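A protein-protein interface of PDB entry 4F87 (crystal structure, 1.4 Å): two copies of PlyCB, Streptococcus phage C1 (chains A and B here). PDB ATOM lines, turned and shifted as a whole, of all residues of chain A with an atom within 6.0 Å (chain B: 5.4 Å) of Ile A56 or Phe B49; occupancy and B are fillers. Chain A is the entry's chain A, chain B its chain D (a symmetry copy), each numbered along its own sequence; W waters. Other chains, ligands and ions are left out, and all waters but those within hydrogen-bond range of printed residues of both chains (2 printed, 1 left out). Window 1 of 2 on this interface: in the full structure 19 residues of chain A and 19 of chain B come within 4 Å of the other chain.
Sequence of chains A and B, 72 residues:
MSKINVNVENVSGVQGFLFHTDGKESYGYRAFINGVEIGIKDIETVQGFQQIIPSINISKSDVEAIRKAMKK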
ATOM      1  N   PHE A  17      11.125  10.263  11.767  1.00  0.00           N
ATOM      2  CA  PHE A  17      11.893   9.517  12.726  1.00  0.00           C
ATOM      3  C   PHE A  17      12.152  10.372  13.949  1.00  0.00           C
ATOM      4  O   PHE A  17      12.175  11.605  13.861  1.00  0.00           O
ATOM      5  CB  PHE A  17      13.247   9.041  12.118  1.00  0.00           C
ATOM      6  CG  PHE A  17      14.102  10.133  11.518  1.00  0.00           C
ATOM      7  CD1 PHE A  17      15.011  10.836  12.296  1.00  0.00           C
ATOM      8  CD2 PHE A  17      14.002  10.459  10.170  1.00  0.00           C
ATOM      9  CE1 PHE A  17      15.781  11.867  11.742  1.00  0.00           C
ATOM     10  CE2 PHE A  17      14.807  11.468   9.612  1.00  0.00           C
ATOM     11  CZ  PHE A  17      15.688  12.158  10.401  1.00  0.00           C
ATOM     12  N   LEU A  18      12.378   9.703  15.065  1.00  0.00           N
ATOM     13  CA  LEU A  18      12.861  10.336  16.285  1.00  0.00           C
ATOM     14  C   LEU A  18      14.390  10.351  16.203  1.00  0.00           C
ATOM     15  O   LEU A  18      14.991   9.429  15.619  1.00  0.00           O
ATOM     16  CB  LEU A  18      12.465   9.499  17.498  1.00  0.00           C
ATOM     17  CG  LEU A  18      10.994   9.581  17.843  1.00  0.00           C
ATOM     18  CD1 LEU A  18      10.555   8.293  18.485  1.00  0.00           C
ATOM     19  CD2 LEU A  18      10.747  10.746  18.809  1.00  0.00           C
ATOM     20  N   PHE A  19      15.021  11.362  16.820  1.00  0.00           N
ATOM     21  CA  PHE A  19      16.466  11.391  16.892  1.00  0.00           C
ATOM     22  C   PHE A  19      16.943  11.941  18.218  1.00  0.00           C
ATOM     23  O   PHE A  19      16.276  12.787  18.847  1.00  0.00           O
ATOM     24  CB  PHE A  19      17.094  12.149  15.695  1.00  0.00           C
ATOM     25  CG  PHE A  19      16.709  13.591  15.479  1.00  0.00           C
ATOM     26  CD1 PHE A  19      17.602  14.619  15.786  1.00  0.00           C
ATOM     27  CD2 PHE A  19      15.497  13.920  14.890  1.00  0.00           C
ATOM     28  CE1 PHE A  19      17.279  15.946  15.520  1.00  0.00           C
ATOM     29  CE2 PHE A  19      15.167  15.252  14.645  1.00  0.00           C
ATOM     30  CZ  PHE A  19      16.065  16.254  14.947  1.00  0.00           C
ATOM     31  N   HIS A  20      18.091  11.437  18.671  1.00  0.00           N
ATOM     32  CA  HIS A  20      18.754  11.908  19.882  1.00  0.00           C
ATOM     33  C   HIS A  20      20.227  11.550  19.762  1.00  0.00           C
ATOM     34  O   HIS A  20      20.594  10.740  18.892  1.00  0.00           O
ATOM     35  CB  HIS A  20      18.160  11.247  21.152  1.00  0.00           C
ATOM     36  CG  HIS A  20      18.554   9.815  21.344  1.00  0.00           C
ATOM     37  ND1 HIS A  20      17.979   8.804  20.586  1.00  0.00           N
ATOM     38  CD2 HIS A  20      19.491   9.269  22.157  1.00  0.00           C
ATOM     39  CE1 HIS A  20      18.564   7.680  20.967  1.00  0.00           C
ATOM     40  NE2 HIS A  20      19.478   7.900  21.915  1.00  0.00           N
ATOM     41  N   THR A  21      21.061  12.109  20.636  1.00  0.00           N
ATOM     42  CA  THR A  21      22.452  11.705  20.718  1.00  0.00           C
ATOM     43  C   THR A  21      22.734  11.086  22.066  1.00  0.00           C
ATOM     44  O   THR A  21      22.204  11.546  23.092  1.00  0.00           O
ATOM     45  CB  THR A  21      23.426  12.884  20.419  1.00  0.00           C
ATOM     46  OG1 THR A  21      24.768  12.401  20.502  1.00  0.00           O
ATOM     47  CG2 THR A  21      23.330  14.038  21.421  1.00  0.00           C
ATOM     48  N   TYR A  27      20.714  16.865  23.331  1.00  0.00           N
ATOM     49  CA  TYR A  27      19.712  17.846  22.951  1.00  0.00           C
ATOM     50  C   TYR A  27      18.320  17.239  23.232  1.00  0.00           C
ATOM     51  O   TYR A  27      17.319  17.701  22.677  1.00  0.00           O
ATOM     52  CB  TYR A  27      19.868  18.319  21.489  1.00  0.00           C
ATOM     53  CG  TYR A  27      19.961  17.182  20.479  1.00  0.00           C
ATOM     54  CD1 TYR A  27      18.818  16.530  20.032  1.00  0.00           C
ATOM     55  CD2 TYR A  27      21.194  16.760  19.984  1.00  0.00           C
ATOM     56  CE1 TYR A  27      18.892  15.483  19.124  1.00  0.00           C
ATOM     57  CE2 TYR A  27      21.279  15.702  19.076  1.00  0.00           C
ATOM     58  CZ  TYR A  27      20.124  15.069  18.662  1.00  0.00           C
ATOM     59  OH  TYR A  27      20.145  14.001  17.803  1.00  0.00           O
ATOM     60  N   PRO A  54      10.679   4.996  13.102  1.00  0.00           N
ATOM     61  CA  PRO A  54      11.999   4.617  13.631  1.00  0.00           C
ATOM     62  C   PRO A  54      12.567   5.671  14.589  1.00  0.00           C
ATOM     63  O   PRO A  54      12.180   6.847  14.553  1.00  0.00           O
ATOM     64  CB  PRO A  54      12.890   4.507  12.385  1.00  0.00           C
ATOM     65  CG  PRO A  54      12.108   5.053  11.270  1.00  0.00           C
ATOM     66  CD  PRO A  54      10.671   5.186  11.639  1.00  0.00           C
ATOM     67  N   SER A  55      13.516   5.227  15.421  1.00  0.00           N
ATOM     68  CA  SER A  55      14.186   6.075  16.395  1.00  0.00           C
ATOM     69  C   SER A  55      15.681   5.818  16.212  1.00  0.00           C
ATOM     70  O   SER A  55      16.159   4.690  16.376  1.00  0.00           O
ATOM     71  CB  SER A  55      13.707   5.687  17.785  1.00  0.00           C
ATOM     72  OG  SER A  55      14.353   6.467  18.776  1.00  0.00           O
ATOM     73  N   ILE A  56      16.390   6.849  15.754  1.00  0.00           N
ATOM     74  CA  ILE A  56      17.805   6.701  15.412  1.00  0.00           C
ATOM     75  C   ILE A  56      18.661   7.700  16.182  1.00  0.00           C
ATOM     76  O   ILE A  56      18.161   8.643  16.816  1.00  0.00           O
ATOM     77  CB  ILE A  56      18.019   6.836  13.874  1.00  0.00           C
ATOM     78  CG1 ILE A  56      17.723   8.277  13.380  1.00  0.00           C
ATOM     79  CG2 ILE A  56      17.192   5.764  13.118  1.00  0.00           C
ATOM     80  CD1 ILE A  56      18.206   8.553  11.910  1.00  0.00           C
ATOM     81  N   ASN A  57      19.975   7.492  16.106  1.00  0.00           N
ATOM     82  CA  ASN A  57      20.920   8.378  16.768  1.00  0.00           C
ATOM     83  C   ASN A  57      21.534   9.340  15.749  1.00  0.00           C
ATOM     84  O   ASN A  57      21.929   8.919  14.648  1.00  0.00           O
ATOM     85  CB  ASN A  57      22.042   7.571  17.399  1.00  0.00           C
ATOM     86  CG  ASN A  57      21.681   6.859  18.673  1.00  0.00           C
ATOM     87  OD1 ASN A  57      22.320   7.047  19.728  1.00  0.00           O
ATOM     88  ND2 ASN A  57      20.763   5.932  18.600  1.00  0.00           N
ATOM     89  N   ILE A  58      21.617  10.628  16.115  1.00  0.00           N
ATOM     90  CA  ILE A  58      22.228  11.665  15.290  1.00  0.00           C
ATOM     91  C   ILE A  58      23.077  12.510  16.219  1.00  0.00           C
ATOM     92  O   ILE A  58      22.568  13.049  17.218  1.00  0.00           O
ATOM     93  CB  ILE A  58      21.185  12.538  14.543  1.00  0.00           C
ATOM     94  CG1 ILE A  58      20.307  11.667  13.621  1.00  0.00           C
ATOM     95  CG2 ILE A  58      21.891  13.642  13.722  1.00  0.00           C
ATOM     96  CD1 ILE A  58      19.276  12.447  12.819  1.00  0.00           C
ATOM     97  N   ILE A  66      21.417  17.293   8.511  1.00  0.00           N
ATOM     98  CA  ILE A  66      20.205  16.495   8.354  1.00  0.00           C
ATOM     99  C   ILE A  66      19.010  17.426   8.125  1.00  0.00           C
ATOM    100  O   ILE A  66      18.164  17.132   7.290  1.00  0.00           O
ATOM    101  CB  ILE A  66      19.990  15.538   9.558  1.00  0.00           C
ATOM    102  CG1 ILE A  66      21.174  14.573   9.762  1.00  0.00           C
ATOM    103  CG2 ILE A  66      18.652  14.789   9.457  1.00  0.00           C
ATOM    104  CD1 ILE A  66      21.574  13.765   8.524  1.00  0.00           C
ATOM    105  N   VAL B  14      12.693   9.034   4.514  1.00  0.00           N
ATOM    106  CA  VAL B  14      14.056   9.201   4.011  1.00  0.00           C
ATOM    107  C   VAL B  14      14.312   8.198   2.896  1.00  0.00           C
ATOM    108  O   VAL B  14      14.123   7.001   3.091  1.00  0.00           O
ATOM    109  CB  VAL B  14      15.098   9.003   5.132  1.00  0.00           C
ATOM    110  CG1 VAL B  14      16.528   9.135   4.594  1.00  0.00           C
ATOM    111  CG2 VAL B  14      14.877   9.992   6.285  1.00  0.00           C
ATOM    112  N   LEU B  18      24.083   6.054   2.348  1.00  0.00           N
ATOM    113  CA  LEU B  18      25.383   6.507   2.816  1.00  0.00           C
ATOM    114  C   LEU B  18      26.429   6.001   1.827  1.00  0.00           C
ATOM    115  O   LEU B  18      26.284   4.903   1.271  1.00  0.00           O
ATOM    116  CB  LEU B  18      25.687   5.903   4.183  1.00  0.00           C
ATOM    117  CG  LEU B  18      24.864   6.489   5.329  1.00  0.00           C
ATOM    118  CD1 LEU B  18      24.654   5.461   6.424  1.00  0.00           C
ATOM    119  CD2 LEU B  18      25.582   7.681   5.947  1.00  0.00           C
ATOM    120  N   ILE B  33      20.367  12.147   0.839  1.00  0.00           N
ATOM    121  CA  ILE B  33      19.139  12.007   1.618  1.00  0.00           C
ATOM    122  C   ILE B  33      18.095  12.844   0.903  1.00  0.00           C
ATOM    123  O   ILE B  33      18.248  14.068   0.794  1.00  0.00           O
ATOM    124  CB  ILE B  33      19.330  12.407   3.109  1.00  0.00           C
ATOM    125  CG1 ILE B  33      20.221  11.361   3.855  1.00  0.00           C
ATOM    126  CG2 ILE B  33      17.937  12.597   3.818  1.00  0.00           C
ATOM    127  CD1 ILE B  33      20.611  11.683   5.261  1.00  0.00           C
ATOM    128  N   GLU B  44      28.363   8.140  15.173  1.00  0.00           N
ATOM    129  CA  GLU B  44      27.054   7.869  15.745  1.00  0.00           C
ATOM    130  C   GLU B  44      25.967   8.072  14.702  1.00  0.00           C
ATOM    131  O   GLU B  44      25.027   7.276  14.616  1.00  0.00           O
ATOM    132  CB  GLU B  44      26.836   8.788  16.942  1.00  0.00           C
ATOM    133  CG  GLU B  44      25.458   8.595  17.550  1.00  0.00           C
ATOM    134  CD  GLU B  44      25.175   9.502  18.722  1.00  0.00           C
ATOM    135  OE1 GLU B  44      25.634  10.666  18.719  1.00  0.00           O
ATOM    136  OE2 GLU B  44      24.405   9.064  19.602  1.00  0.00           O
ATOM    137  N   THR B  45      26.093   9.153  13.898  1.00  0.00           N
ATOM    138  CA  THR B  45      25.093   9.480  12.884  1.00  0.00           C
ATOM    139  C   THR B  45      25.120   8.443  11.774  1.00  0.00           C
ATOM    140  O   THR B  45      24.069   8.077  11.258  1.00  0.00           O
ATOM    141  CB  THR B  45      25.391  10.861  12.324  1.00  0.00           C
ATOM    142  OG1 THR B  45      25.498  11.778  13.431  1.00  0.00           O
ATOM    143  CG2 THR B  45      24.312  11.341  11.341  1.00  0.00           C
ATOM    144  N   VAL B  46      26.313   7.980  11.387  1.00  0.00           N
ATOM    145  CA  VAL B  46      26.409   6.932  10.371  1.00  0.00           C
ATOM    146  C   VAL B  46      25.652   5.695  10.851  1.00  0.00           C
ATOM    147  O   VAL B  46      24.829   5.158  10.107  1.00  0.00           O
ATOM    148  CB  VAL B  46      27.888   6.578  10.120  1.00  0.00           C
ATOM    149  CG1 VAL B  46      28.008   5.350   9.204  1.00  0.00           C
ATOM    150  CG2 VAL B  46      28.621   7.767   9.501  1.00  0.00           C
ATOM    151  N   GLN B  47      25.904   5.264  12.108  1.00  0.00           N
ATOM    152  CA  GLN B  47      25.219   4.067  12.593  1.00  0.00           C
ATOM    153  C   GLN B  47      23.721   4.295  12.719  1.00  0.00           C
ATOM    154  O   GLN B  47      22.942   3.374  12.458  1.00  0.00           O
ATOM    155  CB  GLN B  47      25.848   3.587  13.898  1.00  0.00           C
ATOM    156  CG  GLN B  47      27.277   3.119  13.632  1.00  0.00           C
ATOM    157  CD  GLN B  47      27.749   2.096  14.612  1.00  0.00           C
ATOM    158  OE1 GLN B  47      28.326   2.437  15.596  1.00  0.00           O
ATOM    159  NE2 GLN B  47      27.426   0.819  14.396  1.00  0.00           N
ATOM    160  N   GLY B  48      23.302   5.512  13.096  1.00  0.00           N
ATOM    161  CA  GLY B  48      21.872   5.842  13.168  1.00  0.00           C
ATOM    162  C   GLY B  48      21.216   5.705  11.796  1.00  0.00           C
ATOM    163  O   GLY B  48      20.207   4.995  11.649  1.00  0.00           O
ATOM    164  N   PHE B  49      21.808   6.346  10.758  1.00  0.00           N
ATOM    165  CA  PHE B  49      21.214   6.223   9.422  1.00  0.00           C
ATOM    166  C   PHE B  49      21.340   4.822   8.837  1.00  0.00           C
ATOM    167  O   PHE B  49      20.467   4.447   8.059  1.00  0.00           O
ATOM    168  CB  PHE B  49      21.759   7.293   8.464  1.00  0.00           C
ATOM    169  CG  PHE B  49      21.000   8.585   8.662  1.00  0.00           C
ATOM    170  CD1 PHE B  49      19.810   8.812   7.994  1.00  0.00           C
ATOM    171  CD2 PHE B  49      21.393   9.509   9.638  1.00  0.00           C
ATOM    172  CE1 PHE B  49      19.057   9.963   8.235  1.00  0.00           C
ATOM    173  CE2 PHE B  49      20.642  10.662   9.867  1.00  0.00           C
ATOM    174  CZ  PHE B  49      19.469  10.873   9.176  1.00  0.00           C
ATOM    175  N   GLN B  50      22.342   4.031   9.264  1.00  0.00           N
ATOM    176  CA  GLN B  50      22.426   2.637   8.814  1.00  0.00           C
ATOM    177  C   GLN B  50      21.236   1.796   9.274  1.00  0.00           C
ATOM    178  O   GLN B  50      21.012   0.713   8.729  1.00  0.00           O
ATOM    179  CB  GLN B  50      23.765   2.001   9.221  1.00  0.00           C
ATOM    180  CG  GLN B  50      24.910   2.473   8.347  1.00  0.00           C
ATOM    181  CD  GLN B  50      26.268   2.006   8.803  1.00  0.00           C
ATOM    182  OE1 GLN B  50      26.498   1.688   9.973  1.00  0.00           O
ATOM    183  NE2 GLN B  50      27.241   2.028   7.884  1.00  0.00           N
ATOM    184  N   GLN B  51      20.446   2.297  10.235  1.00  0.00           N
ATOM    185  CA  GLN B  51      19.247   1.552  10.626  1.00  0.00           C
ATOM    186  C   GLN B  51      18.130   1.735   9.608  1.00  0.00           C
ATOM    187  O   GLN B  51      17.176   0.940   9.629  1.00  0.00           O
ATOM    188  CB  GLN B  51      18.725   2.063  11.974  1.00  0.00           C
ATOM    189  CG  GLN B  51      19.696   1.882  13.123  1.00  0.00           C
ATOM    190  CD  GLN B  51      19.011   1.962  14.461  1.00  0.00           C
ATOM    191  OE1 GLN B  51      17.800   2.199  14.574  1.00  0.00           O
ATOM    192  NE2 GLN B  51      19.769   1.695  15.510  1.00  0.00           N
ATOM    193  N   ILE B  52      18.175   2.807   8.774  1.00  0.00           N
ATOM    194  CA  ILE B  52      17.054   3.119   7.878  1.00  0.00           C
ATOM    195  C   ILE B  52      17.414   3.221   6.403  1.00  0.00           C
ATOM    196  O   ILE B  52      16.491   3.176   5.582  1.00  0.00           O
ATOM    197  CB  ILE B  52      16.286   4.382   8.366  1.00  0.00           C
ATOM    198  CG1 ILE B  52      17.183   5.645   8.422  1.00  0.00           C
ATOM    199  CG2 ILE B  52      15.579   4.123   9.714  1.00  0.00           C
ATOM    200  CD1 ILE B  52      16.390   6.990   8.549  1.00  0.00           C
ATOM    201  N   ILE B  53      18.689   3.435   6.049  1.00  0.00           N
ATOM    202  CA  ILE B  53      19.055   3.519   4.636  1.00  0.00           C
ATOM    203  C   ILE B  53      20.269   2.646   4.366  1.00  0.00           C
ATOM    204  O   ILE B  53      21.083   2.416   5.276  1.00  0.00           O
ATOM    205  CB  ILE B  53      19.283   4.965   4.128  1.00  0.00           C
ATOM    206  CG1 ILE B  53      20.371   5.705   4.933  1.00  0.00           C
ATOM    207  CG2 ILE B  53      17.969   5.744   4.024  1.00  0.00           C
ATOM    208  CD1 ILE B  53      20.705   7.108   4.401  1.00  0.00           C
HETATM  209  O   HOH W   1      18.467   2.577  17.824  1.00  0.00           O
HETATM  210  O   HOH W   2      20.374   4.519  16.127  1.00  0.00           O
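The backbone NH (N) of Leu A18 sits at hydrogen-bond distance from the backbone carbonyl oxygen (O) of Pro A54 (2.9 Å).
N of Ile A56 lies within hydrogen-bond range of O of Leu A18, at 2.9 Å.
N of His A20 lies within hydrogen-bond range of O of Ile A56, at 3.4 Å.
The backbone NH (N) of Ile A58 is in hydrogen-bond range of the backbone carbonyl oxygen (O) of His A20 (3.0 Å).
O of Ile A58 lies within hydrogen-bond range of OH of Tyr A27 (2.7 Å).
Of the 12 printed residues of chain A, 8 touch a printed residue of chain B.
Hydrophobic or aromatic side chains of chain A within 4 Å of the printed part of chain B: Phe A17, Pro A54, Ile A56, Ile A58 and Ile A66.
Hydrophobic or aromatic side chains of chain B that line the printed part of chain A: Val B14, Ile B33, Phe B49 and Ile B52.
Among the printed residues, 14 pairs touch across the chains.
OG1 of Thr A21 sits at hydrogen-bond distance from OE1 of Glu B44 (2.6 Å).
OE1 of Gln B51 lies close to O of Ser A55, 3.5 Å away.
OD1 of Asn A57 lies close to OE2 of Glu B44, 2.9 Å away.
Of the printed residues of chain B, Thr A21 touches Glu B44.
Of the printed residues of chain B, Ser A55 touches Gln B51.
Ile A56 touches just these residues of chain B: Gly B48 (3.4 Å), Phe B49 (3.8 Å) and Gln B51 (3.9 Å).
Of the printed residues of chain A, Glu B44 touches Thr A21 and Asn A57.
Of the printed residues of chain A, Thr B45 touches Asn A57 and Ile A58.
Val B46 touches none of the printed residues of chain A.
Of chain A, only Ile A56 (3.8 Å), Ile A58 (3.7 Å) and Ile A66 (3.5 Å) come within 4 Å of Phe B49.
The nearest residue of chain A that does not touch Phe B49 is Phe A17 (4.2 Å).
Phe A17 touches Val B14 (CE2 to CG2, 3.6 Å).
Pro A54 touches Ile B52.
Ile A56 touches Gly B48 (CG2 to O, 3.4 Å).
CD1 of Ile A56 touches CZ of Phe B49, 3.8 Å away.
Gln B51 touches Ile A56.
Asn A57 touches Thr B45 (O to CA, 3.7 Å).
Asn A57 touches Gly B48.
CD1 of Ile A58 touches CE2 of Phe B49, 3.7 Å away.
Ile A66 touches Ile B33 (CD1 to CD1, 3.99 Å).
Ile A66 touches Phe B49 (CD1 to CE2, 3.5 Å).
Position printed for both chains: 18.
Of the 14 pairs that touch across the chains among the printed residues, none has its exchanged pair printed and touching as well.
Water W1 lies within hydrogen-bond range of NE2 of Gln B51 (2.8 Å) and O of Ser A55 (3.4 Å).
Water W2 lies within hydrogen-bond range of ND2 of Asn A57 and NE2 of Gln B51.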
